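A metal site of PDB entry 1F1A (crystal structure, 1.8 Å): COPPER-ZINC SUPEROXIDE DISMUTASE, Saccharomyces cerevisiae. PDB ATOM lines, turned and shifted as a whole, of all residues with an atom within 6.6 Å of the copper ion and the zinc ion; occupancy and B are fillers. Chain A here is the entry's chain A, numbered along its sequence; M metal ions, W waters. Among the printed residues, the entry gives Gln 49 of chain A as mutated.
NE2 of His 72 is in hydrogen-bond range of OD1 of Asp 125 (2.7 Å). NE2 of His 47 lies within hydrogen-bond range of OD2 of Asp 125 (2.7 Å). The side-chain carboxylate (OD2) of Asp 84 lies within hydrogen-bond range of the backbone NH (N) of Gly 73 (2.9 Å). A ring nitrogen (NE2) of His 81 sits at hydrogen-bond distance from the side-chain amino group (NZ) of Lys 137 (3.1 Å). The backbone NH (N) of His 121 lies within hydrogen-bond range of the backbone carbonyl oxygen (O) of Gly 45. The backbone NH (N) of His 72 lies within hydrogen-bond range of the backbone carbonyl oxygen (O) of Leu 136 (2.8 Å). O of Gly 142 sits at hydrogen-bond distance from ND1 of His 121, 2.9 Å away. O of His 47 sits at hydrogen-bond distance from N of Val 119 (2.8 Å).
O of Lys 137 touches the zinc ion, 3.8 Å away. Of the 25 residues printed, 5 come within 4 Å of the zinc ion. The nearest printed residue that does not touch the zinc ion is Gly 73 (4.9 Å).
The copper ion is bound by water W1 (1.9 Å), NE2 of His 64 (2.1 Å), NE2 of His 121 (2.1 Å), ND1 of His 47 (2.1 Å) and water W2 (2.3 Å). The copper ion has five donor atoms within binding distance.
The zinc ion is bound by the side-chain carboxylate (OD1) of Asp 84 (1.9 Å), a ring nitrogen (ND1) of His 64 (1.9 Å), a ring nitrogen (ND1) of His 72 (2.2 Å) and a ring nitrogen (ND1) of His 81 (2.3 Å). Slightly farther from the zinc ion lies the side-chain carboxylate (OD2) of Asp 84 (2.8 Å).
Merely in contact with the copper ion: Gln 49 (3.5 Å). Along chain A the residues within 4 Å of the copper ion span positions 47 to 121.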
ATOM      1  N   GLY A  45     -14.409  18.166 -32.047  1.00  0.00           N
ATOM      2  CA  GLY A  45     -14.476  17.905 -30.614  1.00  0.00           C
ATOM      3  C   GLY A  45     -14.448  16.403 -30.315  1.00  0.00           C
ATOM      4  O   GLY A  45     -15.235  15.653 -30.864  1.00  0.00           O
ATOM      5  N   PHE A  46     -13.606  15.995 -29.370  1.00  0.00           N
ATOM      6  CA  PHE A  46     -13.414  14.603 -28.993  1.00  0.00           C
ATOM      7  C   PHE A  46     -13.541  14.553 -27.458  1.00  0.00           C
ATOM      8  O   PHE A  46     -12.665  15.026 -26.752  1.00  0.00           O
ATOM      9  CB  PHE A  46     -11.982  14.244 -29.447  1.00  0.00           C
ATOM     10  CG  PHE A  46     -11.629  12.796 -29.350  1.00  0.00           C
ATOM     11  CD1 PHE A  46     -12.525  11.806 -29.737  1.00  0.00           C
ATOM     12  CD2 PHE A  46     -10.358  12.419 -28.930  1.00  0.00           C
ATOM     13  CE1 PHE A  46     -12.145  10.456 -29.716  1.00  0.00           C
ATOM     14  CE2 PHE A  46      -9.961  11.083 -28.920  1.00  0.00           C
ATOM     15  CZ  PHE A  46     -10.855  10.103 -29.308  1.00  0.00           C
ATOM     16  N   HIS A  47     -14.651  14.016 -26.944  1.00  0.00           N
ATOM     17  CA  HIS A  47     -14.876  14.024 -25.500  1.00  0.00           C
ATOM     18  C   HIS A  47     -15.418  12.729 -24.924  1.00  0.00           C
ATOM     19  O   HIS A  47     -15.960  11.904 -25.641  1.00  0.00           O
ATOM     20  CB  HIS A  47     -15.884  15.120 -25.130  1.00  0.00           C
ATOM     21  CG  HIS A  47     -15.606  16.452 -25.768  1.00  0.00           C
ATOM     22  ND1 HIS A  47     -16.566  17.173 -26.461  1.00  0.00           N
ATOM     23  CD2 HIS A  47     -14.455  17.161 -25.870  1.00  0.00           C
ATOM     24  CE1 HIS A  47     -16.000  18.249 -26.967  1.00  0.00           C
ATOM     25  NE2 HIS A  47     -14.724  18.270 -26.624  1.00  0.00           N
ATOM     26  N   ILE A  48     -15.267  12.586 -23.612  1.00  0.00           N
ATOM     27  CA  ILE A  48     -15.790  11.447 -22.867  1.00  0.00           C
ATOM     28  C   ILE A  48     -17.000  11.974 -22.105  1.00  0.00           C
ATOM     29  O   ILE A  48     -16.915  13.011 -21.438  1.00  0.00           O
ATOM     30  CB  ILE A  48     -14.757  10.841 -21.881  1.00  0.00           C
ATOM     31  CG1 ILE A  48     -13.556  10.315 -22.654  1.00  0.00           C
ATOM     32  CG2 ILE A  48     -15.382   9.709 -21.066  1.00  0.00           C
ATOM     33  CD1 ILE A  48     -12.541   9.654 -21.793  1.00  0.00           C
ATOM     34  N   GLN A  49     -18.141  11.306 -22.284  1.00  0.00           N
ATOM     35  CA  GLN A  49     -19.410  11.664 -21.652  1.00  0.00           C
ATOM     36  C   GLN A  49     -19.579  10.947 -20.303  1.00  0.00           C
ATOM     37  O   GLN A  49     -18.927   9.938 -20.059  1.00  0.00           O
ATOM     38  CB  GLN A  49     -20.560  11.303 -22.577  1.00  0.00           C
ATOM     39  CG  GLN A  49     -20.389  11.756 -24.003  1.00  0.00           C
ATOM     40  CD  GLN A  49     -20.433  13.271 -24.162  1.00  0.00           C
ATOM     41  OE1 GLN A  49     -19.756  13.832 -25.038  1.00  0.00           O
ATOM     42  NE2 GLN A  49     -21.245  13.941 -23.346  1.00  0.00           N
ATOM     43  N   HIS A  64     -20.388  16.000 -20.475  1.00  0.00           N
ATOM     44  CA  HIS A  64     -19.003  15.591 -20.334  1.00  0.00           C
ATOM     45  C   HIS A  64     -18.754  15.055 -18.925  1.00  0.00           C
ATOM     46  O   HIS A  64     -19.305  15.577 -17.946  1.00  0.00           O
ATOM     47  CB  HIS A  64     -18.088  16.782 -20.571  1.00  0.00           C
ATOM     48  CG  HIS A  64     -18.062  17.248 -21.982  1.00  0.00           C
ATOM     49  ND1 HIS A  64     -17.493  18.435 -22.374  1.00  0.00           N
ATOM     50  CD2 HIS A  64     -18.541  16.671 -23.112  1.00  0.00           C
ATOM     51  CE1 HIS A  64     -17.613  18.581 -23.673  1.00  0.00           C
ATOM     52  NE2 HIS A  64     -18.244  17.520 -24.155  1.00  0.00           N
ATOM     53  N   PHE A  65     -17.937  13.997 -18.830  1.00  0.00           N
ATOM     54  CA  PHE A  65     -17.605  13.399 -17.535  1.00  0.00           C
ATOM     55  C   PHE A  65     -16.876  14.543 -16.783  1.00  0.00           C
ATOM     56  O   PHE A  65     -15.831  15.037 -17.215  1.00  0.00           O
ATOM     57  CB  PHE A  65     -16.715  12.151 -17.737  1.00  0.00           C
ATOM     58  CG  PHE A  65     -16.402  11.399 -16.458  1.00  0.00           C
ATOM     59  CD1 PHE A  65     -17.348  11.263 -15.446  1.00  0.00           C
ATOM     60  CD2 PHE A  65     -15.135  10.853 -16.264  1.00  0.00           C
ATOM     61  CE1 PHE A  65     -17.026  10.611 -14.255  1.00  0.00           C
ATOM     62  CE2 PHE A  65     -14.805  10.201 -15.062  1.00  0.00           C
ATOM     63  CZ  PHE A  65     -15.766  10.078 -14.064  1.00  0.00           C
ATOM     64  N   THR A  71     -15.338  23.818 -15.246  1.00  0.00           N
ATOM     65  CA  THR A  71     -15.880  24.271 -16.516  1.00  0.00           C
ATOM     66  C   THR A  71     -15.114  23.610 -17.655  1.00  0.00           C
ATOM     67  O   THR A  71     -14.035  23.068 -17.460  1.00  0.00           O
ATOM     68  CB  THR A  71     -15.795  25.788 -16.695  1.00  0.00           C
ATOM     69  OG1 THR A  71     -14.444  26.211 -16.474  1.00  0.00           O
ATOM     70  CG2 THR A  71     -16.712  26.500 -15.722  1.00  0.00           C
ATOM     71  N   HIS A  72     -15.705  23.657 -18.851  1.00  0.00           N
ATOM     72  CA  HIS A  72     -15.112  23.061 -20.048  1.00  0.00           C
ATOM     73  C   HIS A  72     -13.812  23.779 -20.442  1.00  0.00           C
ATOM     74  O   HIS A  72     -13.746  24.997 -20.398  1.00  0.00           O
ATOM     75  CB  HIS A  72     -16.118  23.140 -21.207  1.00  0.00           C
ATOM     76  CG  HIS A  72     -15.614  22.558 -22.486  1.00  0.00           C
ATOM     77  ND1 HIS A  72     -15.586  21.201 -22.722  1.00  0.00           N
ATOM     78  CD2 HIS A  72     -15.041  23.143 -23.549  1.00  0.00           C
ATOM     79  CE1 HIS A  72     -15.009  20.981 -23.892  1.00  0.00           C
ATOM     80  NE2 HIS A  72     -14.665  22.153 -24.415  1.00  0.00           N
ATOM     81  N   GLY A  73     -12.811  23.016 -20.858  1.00  0.00           N
ATOM     82  CA  GLY A  73     -11.551  23.631 -21.250  1.00  0.00           C
ATOM     83  C   GLY A  73     -10.777  22.753 -22.198  1.00  0.00           C
ATOM     84  O   GLY A  73     -11.297  21.771 -22.713  1.00  0.00           O
ATOM     85  N   ARG A  80     -10.631  22.087 -16.569  1.00  0.00           N
ATOM     86  CA  ARG A  80     -11.243  21.343 -17.673  1.00  0.00           C
ATOM     87  C   ARG A  80     -12.041  20.203 -17.057  1.00  0.00           C
ATOM     88  O   ARG A  80     -11.916  19.904 -15.863  1.00  0.00           O
ATOM     89  CB  ARG A  80     -10.165  20.720 -18.574  1.00  0.00           C
ATOM     90  CG  ARG A  80      -9.163  19.893 -17.798  1.00  0.00           C
ATOM     91  CD  ARG A  80      -8.239  19.065 -18.679  1.00  0.00           C
ATOM     92  NE  ARG A  80      -8.774  17.732 -18.952  1.00  0.00           N
ATOM     93  CZ  ARG A  80      -8.056  16.677 -19.336  1.00  0.00           C
ATOM     94  NH1 ARG A  80      -6.739  16.812 -19.508  1.00  0.00           N
ATOM     95  NH2 ARG A  80      -8.610  15.477 -19.450  1.00  0.00           N
ATOM     96  N   HIS A  81     -12.915  19.609 -17.865  1.00  0.00           N
ATOM     97  CA  HIS A  81     -13.674  18.444 -17.424  1.00  0.00           C
ATOM     98  C   HIS A  81     -12.709  17.279 -17.623  1.00  0.00           C
ATOM     99  O   HIS A  81     -11.814  17.361 -18.457  1.00  0.00           O
ATOM    100  CB  HIS A  81     -14.884  18.219 -18.327  1.00  0.00           C
ATOM    101  CG  HIS A  81     -15.909  19.302 -18.232  1.00  0.00           C
ATOM    102  ND1 HIS A  81     -16.707  19.661 -19.287  1.00  0.00           N
ATOM    103  CD2 HIS A  81     -16.291  20.057 -17.185  1.00  0.00           C
ATOM    104  CE1 HIS A  81     -17.553  20.597 -18.895  1.00  0.00           C
ATOM    105  NE2 HIS A  81     -17.318  20.855 -17.623  1.00  0.00           N
ATOM    106  N   VAL A  82     -12.881  16.206 -16.866  1.00  0.00           N
ATOM    107  CA  VAL A  82     -12.018  15.036 -17.022  1.00  0.00           C
ATOM    108  C   VAL A  82     -12.127  14.495 -18.469  1.00  0.00           C
ATOM    109  O   VAL A  82     -11.136  14.069 -19.046  1.00  0.00           O
ATOM    110  CB  VAL A  82     -12.411  13.924 -16.036  1.00  0.00           C
ATOM    111  CG1 VAL A  82     -11.691  12.634 -16.369  1.00  0.00           C
ATOM    112  CG2 VAL A  82     -12.100  14.381 -14.616  1.00  0.00           C
ATOM    113  N   GLY A  83     -13.330  14.548 -19.032  1.00  0.00           N
ATOM    114  CA  GLY A  83     -13.559  14.047 -20.375  1.00  0.00           C
ATOM    115  C   GLY A  83     -13.184  14.974 -21.515  1.00  0.00           C
ATOM    116  O   GLY A  83     -13.476  14.687 -22.666  1.00  0.00           O
ATOM    117  N   ASP A  84     -12.521  16.078 -21.180  1.00  0.00           N
ATOM    118  CA  ASP A  84     -12.142  17.042 -22.204  1.00  0.00           C
ATOM    119  C   ASP A  84     -10.855  16.667 -22.924  1.00  0.00           C
ATOM    120  O   ASP A  84      -9.763  16.958 -22.461  1.00  0.00           O
ATOM    121  CB  ASP A  84     -12.039  18.453 -21.609  1.00  0.00           C
ATOM    122  CG  ASP A  84     -13.418  19.110 -21.394  1.00  0.00           C
ATOM    123  OD1 ASP A  84     -14.466  18.566 -21.841  1.00  0.00           O
ATOM    124  OD2 ASP A  84     -13.481  20.194 -20.780  1.00  0.00           O
ATOM    125  N   VAL A 119     -17.412  10.358 -27.463  1.00  0.00           N
ATOM    126  CA  VAL A 119     -18.150  11.003 -28.530  1.00  0.00           C
ATOM    127  C   VAL A 119     -17.224  11.812 -29.435  1.00  0.00           C
ATOM    128  O   VAL A 119     -16.303  12.482 -28.951  1.00  0.00           O
ATOM    129  CB  VAL A 119     -19.244  11.975 -27.944  1.00  0.00           C
ATOM    130  CG1 VAL A 119     -19.679  12.976 -28.992  1.00  0.00           C
ATOM    131  CG2 VAL A 119     -20.448  11.186 -27.478  1.00  0.00           C
ATOM    132  N   HIS A 121     -17.450  14.735 -32.143  1.00  0.00           N
ATOM    133  CA  HIS A 121     -18.386  15.775 -32.532  1.00  0.00           C
ATOM    134  C   HIS A 121     -18.398  16.118 -33.998  1.00  0.00           C
ATOM    135  O   HIS A 121     -17.529  15.695 -34.739  1.00  0.00           O
ATOM    136  CB  HIS A 121     -18.158  17.034 -31.715  1.00  0.00           C
ATOM    137  CG  HIS A 121     -18.733  16.944 -30.349  1.00  0.00           C
ATOM    138  ND1 HIS A 121     -20.080  17.037 -30.117  1.00  0.00           N
ATOM    139  CD2 HIS A 121     -18.159  16.725 -29.146  1.00  0.00           C
ATOM    140  CE1 HIS A 121     -20.318  16.880 -28.820  1.00  0.00           C
ATOM    141  NE2 HIS A 121     -19.169  16.690 -28.219  1.00  0.00           N
ATOM    142  N   ASP A 125     -14.289  22.131 -31.212  1.00  0.00           N
ATOM    143  CA  ASP A 125     -14.392  22.517 -29.820  1.00  0.00           C
ATOM    144  C   ASP A 125     -13.693  23.876 -29.688  1.00  0.00           C
ATOM    145  O   ASP A 125     -12.539  24.028 -30.154  1.00  0.00           O
ATOM    146  CB  ASP A 125     -13.666  21.431 -28.995  1.00  0.00           C
ATOM    147  CG  ASP A 125     -13.814  21.605 -27.480  1.00  0.00           C
ATOM    148  OD1 ASP A 125     -14.252  22.666 -26.989  1.00  0.00           O
ATOM    149  OD2 ASP A 125     -13.469  20.635 -26.773  1.00  0.00           O
ATOM    150  N   LEU A 136     -18.473  27.131 -21.907  1.00  0.00           N
ATOM    151  CA  LEU A 136     -18.016  26.557 -20.635  1.00  0.00           C
ATOM    152  C   LEU A 136     -18.664  25.220 -20.276  1.00  0.00           C
ATOM    153  O   LEU A 136     -18.315  24.607 -19.273  1.00  0.00           O
ATOM    154  CB  LEU A 136     -18.260  27.529 -19.478  1.00  0.00           C
ATOM    155  CG  LEU A 136     -17.547  28.878 -19.537  1.00  0.00           C
ATOM    156  CD1 LEU A 136     -17.956  29.667 -18.305  1.00  0.00           C
ATOM    157  CD2 LEU A 136     -16.042  28.677 -19.614  1.00  0.00           C
ATOM    158  N   LYS A 137     -19.637  24.805 -21.073  1.00  0.00           N
ATOM    159  CA  LYS A 137     -20.325  23.554 -20.856  1.00  0.00           C
ATOM    160  C   LYS A 137     -19.902  22.508 -21.870  1.00  0.00           C
ATOM    161  O   LYS A 137     -19.335  21.476 -21.518  1.00  0.00           O
ATOM    162  CB  LYS A 137     -21.835  23.780 -20.917  1.00  0.00           C
ATOM    163  CG  LYS A 137     -22.447  24.294 -19.596  1.00  0.00           C
ATOM    164  CD  LYS A 137     -22.092  23.349 -18.402  1.00  0.00           C
ATOM    165  CE  LYS A 137     -20.817  23.805 -17.583  1.00  0.00           C
ATOM    166  NZ  LYS A 137     -19.750  22.719 -17.317  1.00  0.00           N
ATOM    167  N   THR A 138     -20.047  22.842 -23.153  1.00  0.00           N
ATOM    168  CA  THR A 138     -19.733  21.905 -24.217  1.00  0.00           C
ATOM    169  C   THR A 138     -18.620  22.335 -25.182  1.00  0.00           C
ATOM    170  O   THR A 138     -18.178  21.530 -26.011  1.00  0.00           O
ATOM    171  CB  THR A 138     -20.989  21.647 -25.078  1.00  0.00           C
ATOM    172  OG1 THR A 138     -21.298  22.841 -25.830  1.00  0.00           O
ATOM    173  CG2 THR A 138     -22.184  21.292 -24.205  1.00  0.00           C
ATOM    174  N   GLY A 139     -18.161  23.573 -25.063  1.00  0.00           N
ATOM    175  CA  GLY A 139     -17.160  24.031 -25.992  1.00  0.00           C
ATOM    176  C   GLY A 139     -17.822  24.277 -27.340  1.00  0.00           C
ATOM    177  O   GLY A 139     -17.140  24.493 -28.331  1.00  0.00           O
ATOM    178  N   ALA A 141     -19.226  22.343 -29.429  1.00  0.00           N
ATOM    179  CA  ALA A 141     -18.810  21.380 -30.458  1.00  0.00           C
ATOM    180  C   ALA A 141     -19.888  20.790 -31.368  1.00  0.00           C
ATOM    181  O   ALA A 141     -19.600  19.970 -32.251  1.00  0.00           O
ATOM    182  CB  ALA A 141     -17.962  20.295 -29.826  1.00  0.00           C
ATOM    183  N   GLY A 142     -21.138  21.129 -31.128  1.00  0.00           N
ATOM    184  CA  GLY A 142     -22.195  20.646 -31.983  1.00  0.00           C
ATOM    185  C   GLY A 142     -22.680  19.234 -31.738  1.00  0.00           C
ATOM    186  O   GLY A 142     -22.457  18.659 -30.662  1.00  0.00           O
ATOM    187  N   ARG A 144     -23.424  14.995 -32.170  1.00  0.00           N
ATOM    188  CA  ARG A 144     -22.642  13.794 -31.891  1.00  0.00           C
ATOM    189  C   ARG A 144     -22.929  12.730 -32.950  1.00  0.00           C
ATOM    190  O   ARG A 144     -23.776  11.851 -32.739  1.00  0.00           O
ATOM    191  CB  ARG A 144     -23.040  13.241 -30.531  1.00  0.00           C
ATOM    192  CG  ARG A 144     -23.056  14.256 -29.421  1.00  0.00           C
ATOM    193  CD  ARG A 144     -23.639  13.659 -28.163  1.00  0.00           C
ATOM    194  NE  ARG A 144     -23.753  14.688 -27.147  1.00  0.00           N
ATOM    195  CZ  ARG A 144     -23.965  14.471 -25.856  1.00  0.00           C
ATOM    196  NH1 ARG A 144     -24.070  13.234 -25.371  1.00  0.00           N
ATOM    197  NH2 ARG A 144     -24.027  15.509 -25.040  1.00  0.00           N
HETATM  198 CU    CU M   1     -18.681  16.986 -26.154  1.00  0.00          CU
HETATM  199 ZN    ZN M   2     -16.117  19.449 -21.487  1.00  0.00          ZN
HETATM  200  O   HOH W   1     -20.455  16.393 -25.714  1.00  0.00           O
HETATM  201  O   HOH W   2     -19.288  19.136 -26.720  1.00  0.00           O
